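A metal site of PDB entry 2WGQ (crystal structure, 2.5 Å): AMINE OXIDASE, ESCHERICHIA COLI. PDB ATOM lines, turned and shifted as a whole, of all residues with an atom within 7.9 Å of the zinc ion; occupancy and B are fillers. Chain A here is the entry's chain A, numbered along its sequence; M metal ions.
Along chain A the residues within 4 Å of the zinc ion span positions 466 to 689.
The backbone NH of Thr 687 sits at hydrogen-bond distance from the backbone carbonyl oxygen of His 526 (2.8 Å).
The backbone carbonyl oxygen (O) of Thr 522 lies within hydrogen-bond range of a ring nitrogen (ND1) of His 524 (2.7 Å).
A ring nitrogen (NE2) of His 689 sits close to the side-chain carboxylate (OE2) of Glu 490 (3.5 Å).
NE2 of His 689 is in hydrogen-bond range of OE1 of Glu 695 (2.7 Å).
The zinc ion is bound by a ring nitrogen (NE2) of His 526 (2.0 Å), a ring nitrogen (NE2) of His 524 (2.1 Å), a ring nitrogen (ND1) of His 689 (2.1 Å) and the side-chain hydroxyl (OH) of Tyr 466 (2.1 Å).
The zinc ion has four donor atoms within binding distance.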
ATOM      1  N   VAL A 367     -13.132 -29.690  29.999  1.00  0.00           N
ATOM      2  CA  VAL A 367     -13.888 -29.015  28.982  1.00  0.00           C
ATOM      3  C   VAL A 367     -14.512 -27.795  29.633  1.00  0.00           C
ATOM      4  O   VAL A 367     -15.671 -27.819  30.087  1.00  0.00           O
ATOM      5  CB  VAL A 367     -14.858 -29.964  28.296  1.00  0.00           C
ATOM      6  CG1 VAL A 367     -15.563 -29.280  27.120  1.00  0.00           C
ATOM      7  CG2 VAL A 367     -14.100 -31.228  27.843  1.00  0.00           C
ATOM      8  N   TYR A 369     -15.481 -23.498  29.820  1.00  0.00           N
ATOM      9  CA  TYR A 369     -16.213 -22.641  28.907  1.00  0.00           C
ATOM     10  C   TYR A 369     -15.801 -21.178  29.003  1.00  0.00           C
ATOM     11  O   TYR A 369     -15.181 -20.756  29.995  1.00  0.00           O
ATOM     12  CB  TYR A 369     -17.743 -22.869  29.057  1.00  0.00           C
ATOM     13  CG  TYR A 369     -18.195 -24.163  28.385  1.00  0.00           C
ATOM     14  CD1 TYR A 369     -17.905 -25.415  28.956  1.00  0.00           C
ATOM     15  CD2 TYR A 369     -18.844 -24.137  27.160  1.00  0.00           C
ATOM     16  CE1 TYR A 369     -18.272 -26.606  28.309  1.00  0.00           C
ATOM     17  CE2 TYR A 369     -19.211 -25.286  26.516  1.00  0.00           C
ATOM     18  CZ  TYR A 369     -18.928 -26.527  27.089  1.00  0.00           C
ATOM     19  OH  TYR A 369     -19.332 -27.664  26.408  1.00  0.00           O
ATOM     20  N   ASN A 465     -23.454 -34.703  27.668  1.00  0.00           N
ATOM     21  CA  ASN A 465     -23.804 -34.302  26.306  1.00  0.00           C
ATOM     22  C   ASN A 465     -22.757 -34.728  25.251  1.00  0.00           C
ATOM     23  O   ASN A 465     -23.071 -35.023  24.093  1.00  0.00           O
ATOM     24  CB  ASN A 465     -23.969 -32.784  26.303  1.00  0.00           C
ATOM     25  CG  ASN A 465     -22.776 -32.095  26.908  1.00  0.00           C
ATOM     26  OD1 ASN A 465     -22.168 -31.210  26.293  1.00  0.00           O
ATOM     27  ND2 ASN A 465     -22.417 -32.510  28.106  1.00  0.00           N
ATOM     28  N   TYR A 466     -21.510 -34.774  25.702  1.00  0.00           N
ATOM     29  CA  TYR A 466     -20.392 -35.080  24.847  1.00  0.00           C
ATOM     30  C   TYR A 466     -19.956 -36.534  24.932  1.00  0.00           C
ATOM     31  O   TYR A 466     -19.933 -37.163  26.025  1.00  0.00           O
ATOM     32  CB  TYR A 466     -19.222 -34.161  25.201  1.00  0.00           C
ATOM     33  CG  TYR A 466     -19.156 -32.846  24.467  1.00  0.00           C
ATOM     34  CD1 TYR A 466     -18.895 -31.665  25.139  1.00  0.00           C
ATOM     35  CD2 TYR A 466     -19.330 -32.780  23.080  1.00  0.00           C
ATOM     36  CE1 TYR A 466     -18.800 -30.439  24.431  1.00  0.00           C
ATOM     37  CE2 TYR A 466     -19.227 -31.577  22.380  1.00  0.00           C
ATOM     38  CZ  TYR A 466     -18.973 -30.417  23.059  1.00  0.00           C
ATOM     39  OH  TYR A 466     -18.885 -29.245  22.346  1.00  0.00           O
ATOM     40  N   TYR A 468     -16.685 -39.036  23.838  1.00  0.00           N
ATOM     41  CA  TYR A 468     -15.268 -39.026  23.485  1.00  0.00           C
ATOM     42  C   TYR A 468     -14.711 -40.380  23.162  1.00  0.00           C
ATOM     43  O   TYR A 468     -15.049 -41.389  23.801  1.00  0.00           O
ATOM     44  CB  TYR A 468     -14.439 -38.454  24.603  1.00  0.00           C
ATOM     45  CG  TYR A 468     -14.887 -37.089  25.008  1.00  0.00           C
ATOM     46  CD1 TYR A 468     -14.589 -35.988  24.231  1.00  0.00           C
ATOM     47  CD2 TYR A 468     -15.656 -36.920  26.140  1.00  0.00           C
ATOM     48  CE1 TYR A 468     -15.018 -34.713  24.568  1.00  0.00           C
ATOM     49  CE2 TYR A 468     -16.106 -35.672  26.502  1.00  0.00           C
ATOM     50  CZ  TYR A 468     -15.780 -34.560  25.715  1.00  0.00           C
ATOM     51  OH  TYR A 468     -16.215 -33.321  26.085  1.00  0.00           O
ATOM     52  N   ALA A 486     -14.202 -36.509  19.496  1.00  0.00           N
ATOM     53  CA  ALA A 486     -15.302 -35.894  20.257  1.00  0.00           C
ATOM     54  C   ALA A 486     -16.534 -35.839  19.376  1.00  0.00           C
ATOM     55  O   ALA A 486     -16.452 -35.417  18.253  1.00  0.00           O
ATOM     56  CB  ALA A 486     -14.916 -34.508  20.655  1.00  0.00           C
ATOM     57  N   THR A 487     -17.671 -36.267  19.860  1.00  0.00           N
ATOM     58  CA  THR A 487     -18.885 -36.151  19.087  1.00  0.00           C
ATOM     59  C   THR A 487     -20.005 -35.958  20.100  1.00  0.00           C
ATOM     60  O   THR A 487     -19.712 -35.623  21.250  1.00  0.00           O
ATOM     61  CB  THR A 487     -19.051 -37.351  18.088  1.00  0.00           C
ATOM     62  OG1 THR A 487     -20.344 -37.327  17.510  1.00  0.00           O
ATOM     63  CG2 THR A 487     -18.836 -38.685  18.750  1.00  0.00           C
ATOM     64  N   ILE A 489     -23.410 -33.923  21.600  1.00  0.00           N
ATOM     65  CA  ILE A 489     -24.294 -32.774  21.659  1.00  0.00           C
ATOM     66  C   ILE A 489     -23.635 -31.589  22.383  1.00  0.00           C
ATOM     67  O   ILE A 489     -23.291 -31.662  23.579  1.00  0.00           O
ATOM     68  CB  ILE A 489     -25.655 -33.111  22.406  1.00  0.00           C
ATOM     69  CG1 ILE A 489     -26.385 -34.379  21.897  1.00  0.00           C
ATOM     70  CG2 ILE A 489     -26.627 -31.913  22.396  1.00  0.00           C
ATOM     71  CD1 ILE A 489     -26.471 -34.539  20.376  1.00  0.00           C
ATOM     72  N   GLU A 490     -23.483 -30.473  21.680  1.00  0.00           N
ATOM     73  CA  GLU A 490     -22.898 -29.301  22.309  1.00  0.00           C
ATOM     74  C   GLU A 490     -23.774 -28.698  23.426  1.00  0.00           C
ATOM     75  O   GLU A 490     -25.007 -28.702  23.361  1.00  0.00           O
ATOM     76  CB  GLU A 490     -22.573 -28.246  21.262  1.00  0.00           C
ATOM     77  CG  GLU A 490     -21.394 -28.591  20.332  1.00  0.00           C
ATOM     78  CD  GLU A 490     -21.367 -27.761  19.039  1.00  0.00           C
ATOM     79  OE1 GLU A 490     -21.965 -26.646  18.998  1.00  0.00           O
ATOM     80  OE2 GLU A 490     -20.756 -28.232  18.053  1.00  0.00           O
ATOM     81  N   ALA A 491     -23.110 -28.202  24.457  1.00  0.00           N
ATOM     82  CA  ALA A 491     -23.707 -27.377  25.471  1.00  0.00           C
ATOM     83  C   ALA A 491     -24.098 -26.028  24.842  1.00  0.00           C
ATOM     84  O   ALA A 491     -23.203 -25.221  24.561  1.00  0.00           O
ATOM     85  CB  ALA A 491     -22.702 -27.152  26.549  1.00  0.00           C
ATOM     86  N   GLY A 521     -23.877 -21.740  20.395  1.00  0.00           N
ATOM     87  CA  GLY A 521     -22.904 -22.736  20.897  1.00  0.00           C
ATOM     88  C   GLY A 521     -21.664 -22.168  21.599  1.00  0.00           C
ATOM     89  O   GLY A 521     -20.638 -21.973  20.980  1.00  0.00           O
ATOM     90  N   THR A 522     -21.749 -21.931  22.906  1.00  0.00           N
ATOM     91  CA  THR A 522     -20.679 -21.223  23.620  1.00  0.00           C
ATOM     92  C   THR A 522     -19.256 -21.788  23.414  1.00  0.00           C
ATOM     93  O   THR A 522     -19.062 -23.029  23.447  1.00  0.00           O
ATOM     94  CB  THR A 522     -20.897 -21.254  25.121  1.00  0.00           C
ATOM     95  OG1 THR A 522     -22.219 -20.765  25.407  1.00  0.00           O
ATOM     96  CG2 THR A 522     -19.856 -20.401  25.826  1.00  0.00           C
ATOM     97  N   THR A 523     -18.294 -20.898  23.231  1.00  0.00           N
ATOM     98  CA  THR A 523     -16.930 -21.281  22.955  1.00  0.00           C
ATOM     99  C   THR A 523     -16.328 -21.910  24.205  1.00  0.00           C
ATOM    100  O   THR A 523     -16.709 -21.560  25.322  1.00  0.00           O
ATOM    101  CB  THR A 523     -16.114 -20.056  22.442  1.00  0.00           C
ATOM    102  OG1 THR A 523     -16.782 -19.494  21.309  1.00  0.00           O
ATOM    103  CG2 THR A 523     -14.748 -20.435  22.012  1.00  0.00           C
ATOM    104  N   HIS A 524     -15.392 -22.831  24.016  1.00  0.00           N
ATOM    105  CA  HIS A 524     -14.760 -23.524  25.122  1.00  0.00           C
ATOM    106  C   HIS A 524     -13.561 -24.260  24.550  1.00  0.00           C
ATOM    107  O   HIS A 524     -13.326 -24.221  23.339  1.00  0.00           O
ATOM    108  CB  HIS A 524     -15.730 -24.569  25.691  1.00  0.00           C
ATOM    109  CG  HIS A 524     -16.302 -25.457  24.638  1.00  0.00           C
ATOM    110  ND1 HIS A 524     -17.218 -25.005  23.708  1.00  0.00           N
ATOM    111  CD2 HIS A 524     -16.077 -26.758  24.331  1.00  0.00           C
ATOM    112  CE1 HIS A 524     -17.534 -25.980  22.876  1.00  0.00           C
ATOM    113  NE2 HIS A 524     -16.863 -27.060  23.235  1.00  0.00           N
ATOM    114  N   GLN A 525     -12.868 -25.018  25.373  1.00  0.00           N
ATOM    115  CA  GLN A 525     -11.830 -25.876  24.852  1.00  0.00           C
ATOM    116  C   GLN A 525     -12.145 -27.355  25.092  1.00  0.00           C
ATOM    117  O   GLN A 525     -13.002 -27.697  25.910  1.00  0.00           O
ATOM    118  CB  GLN A 525     -10.487 -25.511  25.465  1.00  0.00           C
ATOM    119  CG  GLN A 525     -10.184 -24.017  25.482  1.00  0.00           C
ATOM    120  CD  GLN A 525      -8.726 -23.750  25.733  1.00  0.00           C
ATOM    121  OE1 GLN A 525      -7.922 -23.754  24.800  1.00  0.00           O
ATOM    122  NE2 GLN A 525      -8.358 -23.533  27.002  1.00  0.00           N
ATOM    123  N   HIS A 526     -11.461 -28.212  24.364  1.00  0.00           N
ATOM    124  CA  HIS A 526     -11.419 -29.623  24.708  1.00  0.00           C
ATOM    125  C   HIS A 526      -9.944 -29.919  25.014  1.00  0.00           C
ATOM    126  O   HIS A 526      -9.133 -29.856  24.102  1.00  0.00           O
ATOM    127  CB  HIS A 526     -11.903 -30.429  23.522  1.00  0.00           C
ATOM    128  CG  HIS A 526     -13.376 -30.323  23.281  1.00  0.00           C
ATOM    129  ND1 HIS A 526     -14.293 -31.072  23.971  1.00  0.00           N
ATOM    130  CD2 HIS A 526     -14.099 -29.547  22.415  1.00  0.00           C
ATOM    131  CE1 HIS A 526     -15.510 -30.783  23.555  1.00  0.00           C
ATOM    132  NE2 HIS A 526     -15.422 -29.866  22.615  1.00  0.00           N
ATOM    133  N   TYR A 528      -7.153 -32.635  26.508  1.00  0.00           N
ATOM    134  CA  TYR A 528      -6.910 -33.998  26.938  1.00  0.00           C
ATOM    135  C   TYR A 528      -5.485 -34.136  27.439  1.00  0.00           C
ATOM    136  O   TYR A 528      -4.550 -33.594  26.857  1.00  0.00           O
ATOM    137  CB  TYR A 528      -7.145 -34.978  25.794  1.00  0.00           C
ATOM    138  CG  TYR A 528      -8.417 -34.787  24.980  1.00  0.00           C
ATOM    139  CD1 TYR A 528      -9.655 -35.310  25.405  1.00  0.00           C
ATOM    140  CD2 TYR A 528      -8.381 -34.127  23.762  1.00  0.00           C
ATOM    141  CE1 TYR A 528     -10.842 -35.125  24.622  1.00  0.00           C
ATOM    142  CE2 TYR A 528      -9.561 -33.948  22.984  1.00  0.00           C
ATOM    143  CZ  TYR A 528     -10.769 -34.444  23.437  1.00  0.00           C
ATOM    144  OH  TYR A 528     -11.857 -34.263  22.627  1.00  0.00           O
ATOM    145  N   HIS A 613     -10.164 -29.465  14.635  1.00  0.00           N
ATOM    146  CA  HIS A 613     -10.577 -28.209  15.234  1.00  0.00           C
ATOM    147  C   HIS A 613      -9.331 -27.335  15.505  1.00  0.00           C
ATOM    148  O   HIS A 613      -8.184 -27.852  15.508  1.00  0.00           O
ATOM    149  CB  HIS A 613     -11.254 -28.475  16.558  1.00  0.00           C
ATOM    150  CG  HIS A 613     -12.749 -28.566  16.500  1.00  0.00           C
ATOM    151  ND1 HIS A 613     -13.485 -29.107  17.537  1.00  0.00           N
ATOM    152  CD2 HIS A 613     -13.637 -28.179  15.562  1.00  0.00           C
ATOM    153  CE1 HIS A 613     -14.769 -29.056  17.219  1.00  0.00           C
ATOM    154  NE2 HIS A 613     -14.894 -28.498  16.032  1.00  0.00           N
ATOM    155  N   THR A 687      -8.093 -28.245  22.045  1.00  0.00           N
ATOM    156  CA  THR A 687      -8.688 -27.471  20.973  1.00  0.00           C
ATOM    157  C   THR A 687      -9.464 -26.289  21.515  1.00  0.00           C
ATOM    158  O   THR A 687      -9.921 -26.291  22.659  1.00  0.00           O
ATOM    159  CB  THR A 687      -9.670 -28.310  20.146  1.00  0.00           C
ATOM    160  OG1 THR A 687     -10.803 -28.672  20.962  1.00  0.00           O
ATOM    161  CG2 THR A 687      -9.000 -29.567  19.621  1.00  0.00           C
ATOM    162  N   THR A 688      -9.614 -25.274  20.670  1.00  0.00           N
ATOM    163  CA  THR A 688     -10.518 -24.187  20.976  1.00  0.00           C
ATOM    164  C   THR A 688     -11.722 -24.382  20.094  1.00  0.00           C
ATOM    165  O   THR A 688     -11.600 -24.408  18.879  1.00  0.00           O
ATOM    166  CB  THR A 688      -9.835 -22.886  20.738  1.00  0.00           C
ATOM    167  OG1 THR A 688      -8.887 -22.695  21.782  1.00  0.00           O
ATOM    168  CG2 THR A 688     -10.825 -21.728  20.779  1.00  0.00           C
ATOM    169  N   HIS A 689     -12.890 -24.580  20.694  1.00  0.00           N
ATOM    170  CA  HIS A 689     -14.026 -25.011  19.918  1.00  0.00           C
ATOM    171  C   HIS A 689     -14.935 -23.837  19.670  1.00  0.00           C
ATOM    172  O   HIS A 689     -15.613 -23.359  20.570  1.00  0.00           O
ATOM    173  CB  HIS A 689     -14.761 -26.240  20.540  1.00  0.00           C
ATOM    174  CG  HIS A 689     -15.906 -26.771  19.707  1.00  0.00           C
ATOM    175  ND1 HIS A 689     -16.718 -27.798  20.133  1.00  0.00           N
ATOM    176  CD2 HIS A 689     -16.379 -26.401  18.485  1.00  0.00           C
ATOM    177  CE1 HIS A 689     -17.633 -28.049  19.211  1.00  0.00           C
ATOM    178  NE2 HIS A 689     -17.448 -27.217  18.197  1.00  0.00           N
ATOM    179  N   VAL A 690     -14.899 -23.373  18.428  1.00  0.00           N
ATOM    180  CA  VAL A 690     -15.849 -22.359  17.975  1.00  0.00           C
ATOM    181  C   VAL A 690     -16.855 -23.075  17.063  1.00  0.00           C
ATOM    182  O   VAL A 690     -16.492 -23.703  16.052  1.00  0.00           O
ATOM    183  CB  VAL A 690     -15.131 -21.164  17.276  1.00  0.00           C
ATOM    184  CG1 VAL A 690     -16.139 -20.228  16.584  1.00  0.00           C
ATOM    185  CG2 VAL A 690     -14.293 -20.398  18.270  1.00  0.00           C
ATOM    186  N   ALA A 691     -18.115 -23.006  17.474  1.00  0.00           N
ATOM    187  CA  ALA A 691     -19.166 -23.826  16.889  1.00  0.00           C
ATOM    188  C   ALA A 691     -19.615 -23.320  15.542  1.00  0.00           C
ATOM    189  O   ALA A 691     -19.305 -22.178  15.123  1.00  0.00           O
ATOM    190  CB  ALA A 691     -20.324 -23.895  17.818  1.00  0.00           C
ATOM    191  N   GLU A 695     -22.519 -28.463  13.134  1.00  0.00           N
ATOM    192  CA  GLU A 695     -22.308 -29.305  14.322  1.00  0.00           C
ATOM    193  C   GLU A 695     -23.609 -29.448  15.174  1.00  0.00           C
ATOM    194  O   GLU A 695     -23.585 -29.944  16.307  1.00  0.00           O
ATOM    195  CB  GLU A 695     -21.092 -28.818  15.166  1.00  0.00           C
ATOM    196  CG  GLU A 695     -19.788 -28.642  14.392  1.00  0.00           C
ATOM    197  CD  GLU A 695     -18.717 -27.824  15.142  1.00  0.00           C
ATOM    198  OE1 GLU A 695     -19.071 -26.975  16.017  1.00  0.00           O
ATOM    199  OE2 GLU A 695     -17.496 -28.004  14.819  1.00  0.00           O
ATOM    200  N   MET A 699     -22.786 -33.181  16.810  1.00  0.00           N
ATOM    201  CA  MET A 699     -21.447 -32.829  16.226  1.00  0.00           C
ATOM    202  C   MET A 699     -20.717 -33.979  15.575  1.00  0.00           C
ATOM    203  O   MET A 699     -20.269 -34.897  16.254  1.00  0.00           O
ATOM    204  CB  MET A 699     -20.515 -32.213  17.274  1.00  0.00           C
ATOM    205  CG  MET A 699     -19.198 -31.711  16.676  1.00  0.00           C
ATOM    206  SD  MET A 699     -18.144 -30.988  17.961  1.00  0.00           S
ATOM    207  CE  MET A 699     -17.528 -32.503  18.789  1.00  0.00           C
ATOM    208  N   GLU A 702     -14.993 -34.971  15.759  1.00  0.00           N
ATOM    209  CA  GLU A 702     -13.735 -34.259  15.540  1.00  0.00           C
ATOM    210  C   GLU A 702     -12.552 -34.983  16.194  1.00  0.00           C
ATOM    211  O   GLU A 702     -12.700 -35.618  17.244  1.00  0.00           O
ATOM    212  CB  GLU A 702     -13.853 -32.844  16.092  1.00  0.00           C
ATOM    213  CG  GLU A 702     -14.994 -32.055  15.444  1.00  0.00           C
ATOM    214  CD  GLU A 702     -14.570 -31.310  14.190  1.00  0.00           C
ATOM    215  OE1 GLU A 702     -13.409 -31.434  13.763  1.00  0.00           O
ATOM    216  OE2 GLU A 702     -15.417 -30.571  13.633  1.00  0.00           O
HETATM  217 ZN    ZN M   1     -16.902 -28.703  21.988  1.00  0.00          ZN
